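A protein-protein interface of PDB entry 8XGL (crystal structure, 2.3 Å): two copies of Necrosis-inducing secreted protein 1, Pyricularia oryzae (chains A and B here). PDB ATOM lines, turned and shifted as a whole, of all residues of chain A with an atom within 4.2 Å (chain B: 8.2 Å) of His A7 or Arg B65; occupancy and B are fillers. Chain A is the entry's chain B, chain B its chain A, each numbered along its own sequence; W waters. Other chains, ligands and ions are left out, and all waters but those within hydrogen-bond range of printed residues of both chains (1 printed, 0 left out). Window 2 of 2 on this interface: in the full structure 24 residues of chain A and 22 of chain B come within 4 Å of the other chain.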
ATOM      1  N   HIS A   7      21.142  18.877  16.707  1.00  0.00           N
ATOM      2  CA  HIS A   7      21.687  18.648  15.339  1.00  0.00           C
ATOM      3  C   HIS A   7      23.003  17.858  15.342  1.00  0.00           C
ATOM      4  O   HIS A   7      23.407  17.337  14.303  1.00  0.00           O
ATOM      5  CB  HIS A   7      21.892  19.990  14.621  1.00  0.00           C
ATOM      6  CG  HIS A   7      20.805  20.336  13.649  1.00  0.00           C
ATOM      7  ND1 HIS A   7      21.015  21.167  12.569  1.00  0.00           N
ATOM      8  CD2 HIS A   7      19.500  19.975  13.596  1.00  0.00           C
ATOM      9  CE1 HIS A   7      19.889  21.299  11.890  1.00  0.00           C
ATOM     10  NE2 HIS A   7      18.954  20.586  12.492  1.00  0.00           N
ATOM     11  N   HIS A   8      23.672  17.765  16.489  1.00  0.00           N
ATOM     12  CA  HIS A   8      24.943  17.044  16.582  1.00  0.00           C
ATOM     13  C   HIS A   8      25.036  16.309  17.908  1.00  0.00           C
ATOM     14  O   HIS A   8      26.047  16.343  18.610  1.00  0.00           O
ATOM     15  CB  HIS A   8      26.118  17.987  16.374  1.00  0.00           C
ATOM     16  CG  HIS A   8      26.333  18.328  14.938  1.00  0.00           C
ATOM     17  ND1 HIS A   8      27.283  17.705  14.160  1.00  0.00           N
ATOM     18  CD2 HIS A   8      25.674  19.181  14.120  1.00  0.00           C
ATOM     19  CE1 HIS A   8      27.224  18.186  12.932  1.00  0.00           C
ATOM     20  NE2 HIS A   8      26.254  19.081  12.880  1.00  0.00           N
ATOM     21  N   HIS A   9      23.958  15.611  18.241  1.00  0.00           N
ATOM     22  CA  HIS A   9      23.902  14.741  19.399  1.00  0.00           C
ATOM     23  C   HIS A   9      23.044  13.538  19.038  1.00  0.00           C
ATOM     24  O   HIS A   9      22.300  13.557  18.055  1.00  0.00           O
ATOM     25  CB  HIS A   9      23.347  15.484  20.616  1.00  0.00           C
ATOM     26  CG  HIS A   9      21.935  15.947  20.448  1.00  0.00           C
ATOM     27  ND1 HIS A   9      21.609  17.153  19.865  1.00  0.00           N
ATOM     28  CD2 HIS A   9      20.760  15.366  20.791  1.00  0.00           C
ATOM     29  CE1 HIS A   9      20.297  17.297  19.856  1.00  0.00           C
ATOM     30  NE2 HIS A   9      19.758  16.226  20.411  1.00  0.00           N
ATOM     31  N   ASN A  38      26.239  15.299  11.292  1.00  0.00           N
ATOM     32  CA  ASN A  38      24.846  15.653  11.524  1.00  0.00           C
ATOM     33  C   ASN A  38      24.067  14.409  11.920  1.00  0.00           C
ATOM     34  O   ASN A  38      24.238  13.338  11.334  1.00  0.00           O
ATOM     35  CB  ASN A  38      24.230  16.275  10.270  1.00  0.00           C
ATOM     36  CG  ASN A  38      24.248  15.328   9.085  1.00  0.00           C
ATOM     37  OD1 ASN A  38      25.295  15.095   8.483  1.00  0.00           O
ATOM     38  ND2 ASN A  38      23.087  14.770   8.751  1.00  0.00           N
ATOM     39  N   TYR A  39      23.198  14.556  12.915  1.00  0.00           N
ATOM     40  CA  TYR A  39      22.476  13.417  13.465  1.00  0.00           C
ATOM     41  C   TYR A  39      21.108  13.872  13.949  1.00  0.00           C
ATOM     42  O   TYR A  39      21.011  14.798  14.758  1.00  0.00           O
ATOM     43  CB  TYR A  39      23.283  12.789  14.601  1.00  0.00           C
ATOM     44  CG  TYR A  39      22.842  11.403  14.996  1.00  0.00           C
ATOM     45  CD1 TYR A  39      21.630  11.200  15.641  1.00  0.00           C
ATOM     46  CD2 TYR A  39      23.641  10.297  14.731  1.00  0.00           C
ATOM     47  CE1 TYR A  39      21.221   9.937  16.007  1.00  0.00           C
ATOM     48  CE2 TYR A  39      23.242   9.027  15.095  1.00  0.00           C
ATOM     49  CZ  TYR A  39      22.030   8.852  15.733  1.00  0.00           C
ATOM     50  OH  TYR A  39      21.617   7.594  16.107  1.00  0.00           O
ATOM     51  N   ASP A  40      20.059  13.233  13.441  1.00  0.00           N
ATOM     52  CA  ASP A  40      18.692  13.474  13.883  1.00  0.00           C
ATOM     53  C   ASP A  40      18.164  12.239  14.601  1.00  0.00           C
ATOM     54  O   ASP A  40      18.257  11.128  14.072  1.00  0.00           O
ATOM     55  CB  ASP A  40      17.774  13.802  12.702  1.00  0.00           C
ATOM     56  CG  ASP A  40      18.228  15.015  11.925  1.00  0.00           C
ATOM     57  OD1 ASP A  40      18.510  16.056  12.554  1.00  0.00           O
ATOM     58  OD2 ASP A  40      18.300  14.927  10.681  1.00  0.00           O
ATOM     59  N   PHE A  72      11.428  14.828  17.350  1.00  0.00           N
ATOM     60  CA  PHE A  72      11.848  15.789  16.341  1.00  0.00           C
ATOM     61  C   PHE A  72      10.923  16.997  16.325  1.00  0.00           C
ATOM     62  O   PHE A  72       9.706  16.862  16.482  1.00  0.00           O
ATOM     63  CB  PHE A  72      11.876  15.154  14.951  1.00  0.00           C
ATOM     64  CG  PHE A  72      12.586  15.988  13.923  1.00  0.00           C
ATOM     65  CD1 PHE A  72      13.959  15.895  13.771  1.00  0.00           C
ATOM     66  CD2 PHE A  72      11.887  16.871  13.119  1.00  0.00           C
ATOM     67  CE1 PHE A  72      14.619  16.659  12.832  1.00  0.00           C
ATOM     68  CE2 PHE A  72      12.545  17.639  12.179  1.00  0.00           C
ATOM     69  CZ  PHE A  72      13.913  17.534  12.036  1.00  0.00           C
ATOM     70  N   LEU A 110      18.499   9.679  11.477  1.00  0.00           N
ATOM     71  CA  LEU A 110      19.165   9.988  10.220  1.00  0.00           C
ATOM     72  C   LEU A 110      20.549  10.516  10.571  1.00  0.00           C
ATOM     73  O   LEU A 110      20.689  11.310  11.507  1.00  0.00           O
ATOM     74  CB  LEU A 110      18.391  11.034   9.396  1.00  0.00           C
ATOM     75  CG  LEU A 110      19.006  11.470   8.056  1.00  0.00           C
ATOM     76  CD1 LEU A 110      17.923  11.819   7.041  1.00  0.00           C
ATOM     77  CD2 LEU A 110      19.963  12.652   8.222  1.00  0.00           C
ATOM     78  N   VAL B  44       7.620  10.007   8.762  1.00  0.00           N
ATOM     79  CA  VAL B  44       8.228   9.956   7.443  1.00  0.00           C
ATOM     80  C   VAL B  44       9.335  10.997   7.373  1.00  0.00           C
ATOM     81  O   VAL B  44       9.082  12.195   7.548  1.00  0.00           O
ATOM     82  CB  VAL B  44       7.192  10.188   6.335  1.00  0.00           C
ATOM     83  CG1 VAL B  44       7.858  10.094   4.979  1.00  0.00           C
ATOM     84  CG2 VAL B  44       6.060   9.176   6.475  1.00  0.00           C
ATOM     85  N   VAL B  45      10.554  10.539   7.123  1.00  0.00           N
ATOM     86  CA  VAL B  45      11.680  11.423   6.850  1.00  0.00           C
ATOM     87  C   VAL B  45      11.709  11.700   5.357  1.00  0.00           C
ATOM     88  O   VAL B  45      11.536  10.790   4.537  1.00  0.00           O
ATOM     89  CB  VAL B  45      13.007  10.806   7.331  1.00  0.00           C
ATOM     90  CG1 VAL B  45      13.276   9.493   6.626  1.00  0.00           C
ATOM     91  CG2 VAL B  45      14.162  11.763   7.084  1.00  0.00           C
ATOM     92  N   TRP B  46      11.924  12.961   4.998  1.00  0.00           N
ATOM     93  CA  TRP B  46      11.959  13.389   3.607  1.00  0.00           C
ATOM     94  C   TRP B  46      13.392  13.715   3.223  1.00  0.00           C
ATOM     95  O   TRP B  46      14.045  14.537   3.875  1.00  0.00           O
ATOM     96  CB  TRP B  46      11.058  14.600   3.384  1.00  0.00           C
ATOM     97  CG  TRP B  46       9.630  14.285   3.622  1.00  0.00           C
ATOM     98  CD1 TRP B  46       8.925  14.514   4.765  1.00  0.00           C
ATOM     99  CD2 TRP B  46       8.723  13.657   2.707  1.00  0.00           C
ATOM    100  NE1 TRP B  46       7.632  14.075   4.616  1.00  0.00           N
ATOM    101  CE2 TRP B  46       7.483  13.544   3.362  1.00  0.00           C
ATOM    102  CE3 TRP B  46       8.839  13.184   1.396  1.00  0.00           C
ATOM    103  CZ2 TRP B  46       6.364  12.982   2.751  1.00  0.00           C
ATOM    104  CZ3 TRP B  46       7.730  12.627   0.791  1.00  0.00           C
ATOM    105  CH2 TRP B  46       6.508  12.529   1.470  1.00  0.00           C
ATOM    106  N   GLY B  47      13.869  13.078   2.167  1.00  0.00           N
ATOM    107  CA  GLY B  47      15.234  13.257   1.730  1.00  0.00           C
ATOM    108  C   GLY B  47      15.294  13.655   0.273  1.00  0.00           C
ATOM    109  O   GLY B  47      14.435  13.297  -0.532  1.00  0.00           O
ATOM    110  N   LEU B  48      16.330  14.417  -0.052  1.00  0.00           N
ATOM    111  CA  LEU B  48      16.635  14.805  -1.420  1.00  0.00           C
ATOM    112  C   LEU B  48      17.986  14.207  -1.778  1.00  0.00           C
ATOM    113  O   LEU B  48      19.002  14.552  -1.164  1.00  0.00           O
ATOM    114  CB  LEU B  48      16.639  16.326  -1.566  1.00  0.00           C
ATOM    115  CG  LEU B  48      16.563  16.811  -3.007  1.00  0.00           C
ATOM    116  CD1 LEU B  48      15.187  16.494  -3.571  1.00  0.00           C
ATOM    117  CD2 LEU B  48      16.852  18.293  -3.065  1.00  0.00           C
ATOM    118  N   ALA B  49      17.998  13.311  -2.757  1.00  0.00           N
ATOM    119  CA  ALA B  49      19.165  12.504  -3.068  1.00  0.00           C
ATOM    120  C   ALA B  49      19.609  12.685  -4.512  1.00  0.00           C
ATOM    121  O   ALA B  49      18.807  13.043  -5.382  1.00  0.00           O
ATOM    122  CB  ALA B  49      18.874  11.017  -2.820  1.00  0.00           C
ATOM    123  N   VAL B  62      18.764   8.405   2.285  1.00  0.00           N
ATOM    124  CA  VAL B  62      17.735   9.246   1.685  1.00  0.00           C
ATOM    125  C   VAL B  62      18.284  10.574   1.185  1.00  0.00           C
ATOM    126  O   VAL B  62      17.523  11.379   0.636  1.00  0.00           O
ATOM    127  CB  VAL B  62      16.558   9.494   2.657  1.00  0.00           C
ATOM    128  CG1 VAL B  62      16.024   8.176   3.212  1.00  0.00           C
ATOM    129  CG2 VAL B  62      16.959  10.453   3.783  1.00  0.00           C
ATOM    130  N   GLY B  63      19.578  10.831   1.355  1.00  0.00           N
ATOM    131  CA  GLY B  63      20.173  12.071   0.898  1.00  0.00           C
ATOM    132  C   GLY B  63      20.094  13.171   1.934  1.00  0.00           C
ATOM    133  O   GLY B  63      20.133  12.904   3.137  1.00  0.00           O
ATOM    134  N   ARG B  64      19.984  14.414   1.478  1.00  0.00           N
ATOM    135  CA  ARG B  64      19.865  15.537   2.396  1.00  0.00           C
ATOM    136  C   ARG B  64      18.481  15.534   3.034  1.00  0.00           C
ATOM    137  O   ARG B  64      17.467  15.436   2.338  1.00  0.00           O
ATOM    138  CB  ARG B  64      20.111  16.849   1.652  1.00  0.00           C
ATOM    139  CG  ARG B  64      19.726  18.092   2.432  1.00  0.00           C
ATOM    140  CD  ARG B  64      20.090  19.358   1.677  1.00  0.00           C
ATOM    141  NE  ARG B  64      20.172  20.505   2.573  1.00  0.00           N
ATOM    142  CZ  ARG B  64      20.166  21.770   2.180  1.00  0.00           C
ATOM    143  NH1 ARG B  64      20.103  22.098   0.900  1.00  0.00           N
ATOM    144  NH2 ARG B  64      20.221  22.733   3.096  1.00  0.00           N
ATOM    145  N   ARG B  65      18.436  15.639   4.360  1.00  0.00           N
ATOM    146  CA  ARG B  65      17.158  15.676   5.060  1.00  0.00           C
ATOM    147  C   ARG B  65      16.500  17.029   4.833  1.00  0.00           C
ATOM    148  O   ARG B  65      17.059  18.067   5.202  1.00  0.00           O
ATOM    149  CB  ARG B  65      17.352  15.421   6.551  1.00  0.00           C
ATOM    150  CG  ARG B  65      16.051  15.378   7.354  1.00  0.00           C
ATOM    151  CD  ARG B  65      16.267  15.883   8.771  1.00  0.00           C
ATOM    152  NE  ARG B  65      16.011  17.314   8.871  1.00  0.00           N
ATOM    153  CZ  ARG B  65      16.672  18.157   9.654  1.00  0.00           C
ATOM    154  NH1 ARG B  65      17.663  17.754  10.434  1.00  0.00           N
ATOM    155  NH2 ARG B  65      16.331  19.443   9.654  1.00  0.00           N
ATOM    156  N   ILE B  66      15.316  17.022   4.224  1.00  0.00           N
ATOM    157  CA  ILE B  66      14.589  18.254   3.938  1.00  0.00           C
ATOM    158  C   ILE B  66      13.290  18.361   4.715  1.00  0.00           C
ATOM    159  O   ILE B  66      12.619  19.405   4.634  1.00  0.00           O
ATOM    160  CB  ILE B  66      14.331  18.414   2.426  1.00  0.00           C
ATOM    161  CG1 ILE B  66      13.349  17.360   1.903  1.00  0.00           C
ATOM    162  CG2 ILE B  66      15.648  18.321   1.665  1.00  0.00           C
ATOM    163  CD1 ILE B  66      12.948  17.586   0.452  1.00  0.00           C
ATOM    164  N   GLY B  67      12.917  17.336   5.473  1.00  0.00           N
ATOM    165  CA  GLY B  67      11.727  17.409   6.305  1.00  0.00           C
ATOM    166  C   GLY B  67      11.586  16.144   7.126  1.00  0.00           C
ATOM    167  O   GLY B  67      12.260  15.136   6.886  1.00  0.00           O
ATOM    168  N   TYR B  68      10.702  16.222   8.115  1.00  0.00           N
ATOM    169  CA  TYR B  68      10.260  15.051   8.858  1.00  0.00           C
ATOM    170  C   TYR B  68       8.808  15.253   9.257  1.00  0.00           C
ATOM    171  O   TYR B  68       8.452  16.321   9.761  1.00  0.00           O
ATOM    172  CB  TYR B  68      11.107  14.803  10.109  1.00  0.00           C
ATOM    173  CG  TYR B  68      10.635  13.588  10.874  1.00  0.00           C
ATOM    174  CD1 TYR B  68      10.853  12.309  10.382  1.00  0.00           C
ATOM    175  CD2 TYR B  68       9.942  13.721  12.072  1.00  0.00           C
ATOM    176  CE1 TYR B  68      10.415  11.196  11.069  1.00  0.00           C
ATOM    177  CE2 TYR B  68       9.500  12.614  12.766  1.00  0.00           C
ATOM    178  CZ  TYR B  68       9.737  11.356  12.259  1.00  0.00           C
ATOM    179  OH  TYR B  68       9.298  10.250  12.947  1.00  0.00           O
ATOM    180  N   THR B  91       9.293  21.020   1.790  1.00  0.00           N
ATOM    181  CA  THR B  91       9.995  22.153   1.195  1.00  0.00           C
ATOM    182  C   THR B  91      11.428  21.753   0.877  1.00  0.00           C
ATOM    183  O   THR B  91      12.128  21.208   1.736  1.00  0.00           O
ATOM    184  CB  THR B  91      10.003  23.379   2.125  1.00  0.00           C
ATOM    185  OG1 THR B  91       8.670  23.668   2.566  1.00  0.00           O
ATOM    186  CG2 THR B  91      10.579  24.611   1.402  1.00  0.00           C
ATOM    187  N   VAL B  92      11.853  22.008  -0.352  1.00  0.00           N
ATOM    188  CA  VAL B  92      13.277  21.927  -0.689  1.00  0.00           C
ATOM    189  C   VAL B  92      13.953  23.222  -0.244  1.00  0.00           C
ATOM    190  O   VAL B  92      13.485  24.311  -0.613  1.00  0.00           O
ATOM    191  CB  VAL B  92      13.469  21.695  -2.185  1.00  0.00           C
ATOM    192  CG1 VAL B  92      14.935  21.882  -2.569  1.00  0.00           C
ATOM    193  CG2 VAL B  92      12.995  20.302  -2.576  1.00  0.00           C
ATOM    194  N   PRO B  93      15.026  23.154   0.546  1.00  0.00           N
ATOM    195  CA  PRO B  93      15.645  24.386   1.055  1.00  0.00           C
ATOM    196  C   PRO B  93      16.032  25.340  -0.065  1.00  0.00           C
ATOM    197  O   PRO B  93      16.394  24.929  -1.169  1.00  0.00           O
ATOM    198  CB  PRO B  93      16.884  23.889   1.809  1.00  0.00           C
ATOM    199  CG  PRO B  93      16.708  22.433   2.006  1.00  0.00           C
ATOM    200  CD  PRO B  93      15.572  21.940   1.177  1.00  0.00           C
ATOM    201  N   GLN B  96      19.319  24.947  -2.138  1.00  0.00           N
ATOM    202  CA  GLN B  96      19.587  23.739  -2.907  1.00  0.00           C
ATOM    203  C   GLN B  96      19.970  24.091  -4.338  1.00  0.00           C
ATOM    204  O   GLN B  96      19.328  24.926  -4.984  1.00  0.00           O
ATOM    205  CB  GLN B  96      18.371  22.817  -2.920  1.00  0.00           C
ATOM    206  CG  GLN B  96      18.662  21.453  -3.528  1.00  0.00           C
ATOM    207  CD  GLN B  96      19.659  20.662  -2.704  1.00  0.00           C
ATOM    208  OE1 GLN B  96      19.634  20.707  -1.475  1.00  0.00           O
ATOM    209  NE2 GLN B  96      20.552  19.945  -3.377  1.00  0.00           N
ATOM    210  N   ILE B 104      12.984  11.221  -1.621  1.00  0.00           N
ATOM    211  CA  ILE B 104      12.901   9.940  -0.939  1.00  0.00           C
ATOM    212  C   ILE B 104      12.104  10.114   0.343  1.00  0.00           C
ATOM    213  O   ILE B 104      12.411  10.987   1.164  1.00  0.00           O
ATOM    214  CB  ILE B 104      14.300   9.368  -0.659  1.00  0.00           C
ATOM    215  CG1 ILE B 104      15.070   9.318  -1.978  1.00  0.00           C
ATOM    216  CG2 ILE B 104      14.190   7.988  -0.029  1.00  0.00           C
ATOM    217  CD1 ILE B 104      16.198   8.341  -2.008  1.00  0.00           C
HETATM  218  O   HOH W   1      20.360  16.185   9.555  1.00  0.00           O
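NH1 of Arg B65 lies within salt-bridge range of OD1 of Asp A40 (2.8 Å).
The backbone NH (N) of Leu B48 lies within hydrogen-bond range of the backbone carbonyl oxygen (O) of Val B62 (3.3 Å).
N of Tyr A39 sits at hydrogen-bond distance from O of His A7 (3.1 Å).
O of Leu A110 sits at hydrogen-bond distance from N of Asp A40 (2.8 Å).
Arg B65 touches His A7.
Arg B65 touches Phe A72.
CD2 of Phe A72 touches CB of Tyr B68, 3.7 Å away.
CD1 of Leu A110 touches CG2 of Val B45 (3.8 Å).
Val B62 touches Leu A110.
Arg B65 touches Leu A110 (CB to CD1, 3.7 Å).
His A7 touches just one residue of chain B: Arg B65.
Of the printed residues of chain B, Asp A40 touches Arg B65 (2.8 Å).
Printed residues of chain B within 4 Å of Phe A72: Arg B65 and Tyr B68.
Of the printed residues of chain B, Leu A110 touches Val B45 (3.8 Å), Val B62 (3.7 Å) and Arg B65 (3.7 Å).
Of chain A, only His A7, Asp A40, Phe A72 and Leu A110 come within 4 Å of Arg B65.
Printed residues of chain A within 4 Å of Tyr B68: Phe A72.
Thr B91 touches none of the printed residues of chain A.
The nearest printed residue of chain B that does not touch His A7 is Arg B64 (8.9 Å).
The nearest printed residue of chain A that does not touch Arg B65 is Asn A38 (6.2 Å).
Of the 18 printed residues of chain B, 4 touch a printed residue of chain A.
Printed residues of chain B that touch a printed residue of chain A: Val B45, Val B62, Arg B65 and Tyr B68.
Hydrophobic or aromatic side chains of chain B that line the printed part of chain A: Val B45, Val B62 and Tyr B68.
Of the 8 printed residues of chain A, 4 touch a printed residue of chain B.
Hydrophobic or aromatic side chains of chain A that line the printed part of chain B: His A7, Phe A72 and Leu A110.
Among the printed residues, 7 pairs touch across the chains.
Among the printed residues, Asp or Glu carboxylates within 4 Å of a Lys or Arg side-chain nitrogen of the other chain: Asp A40 with Arg B65 (2.8 Å).
No position is printed for both chains.
Of the 7 pairs that touch across the chains among the printed residues, none has its exchanged pair printed and touching as well.
Water W1 lies within hydrogen-bond range of OD2 of Asp A40, ND2 of Asn A38 and NH1 of Arg B65.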
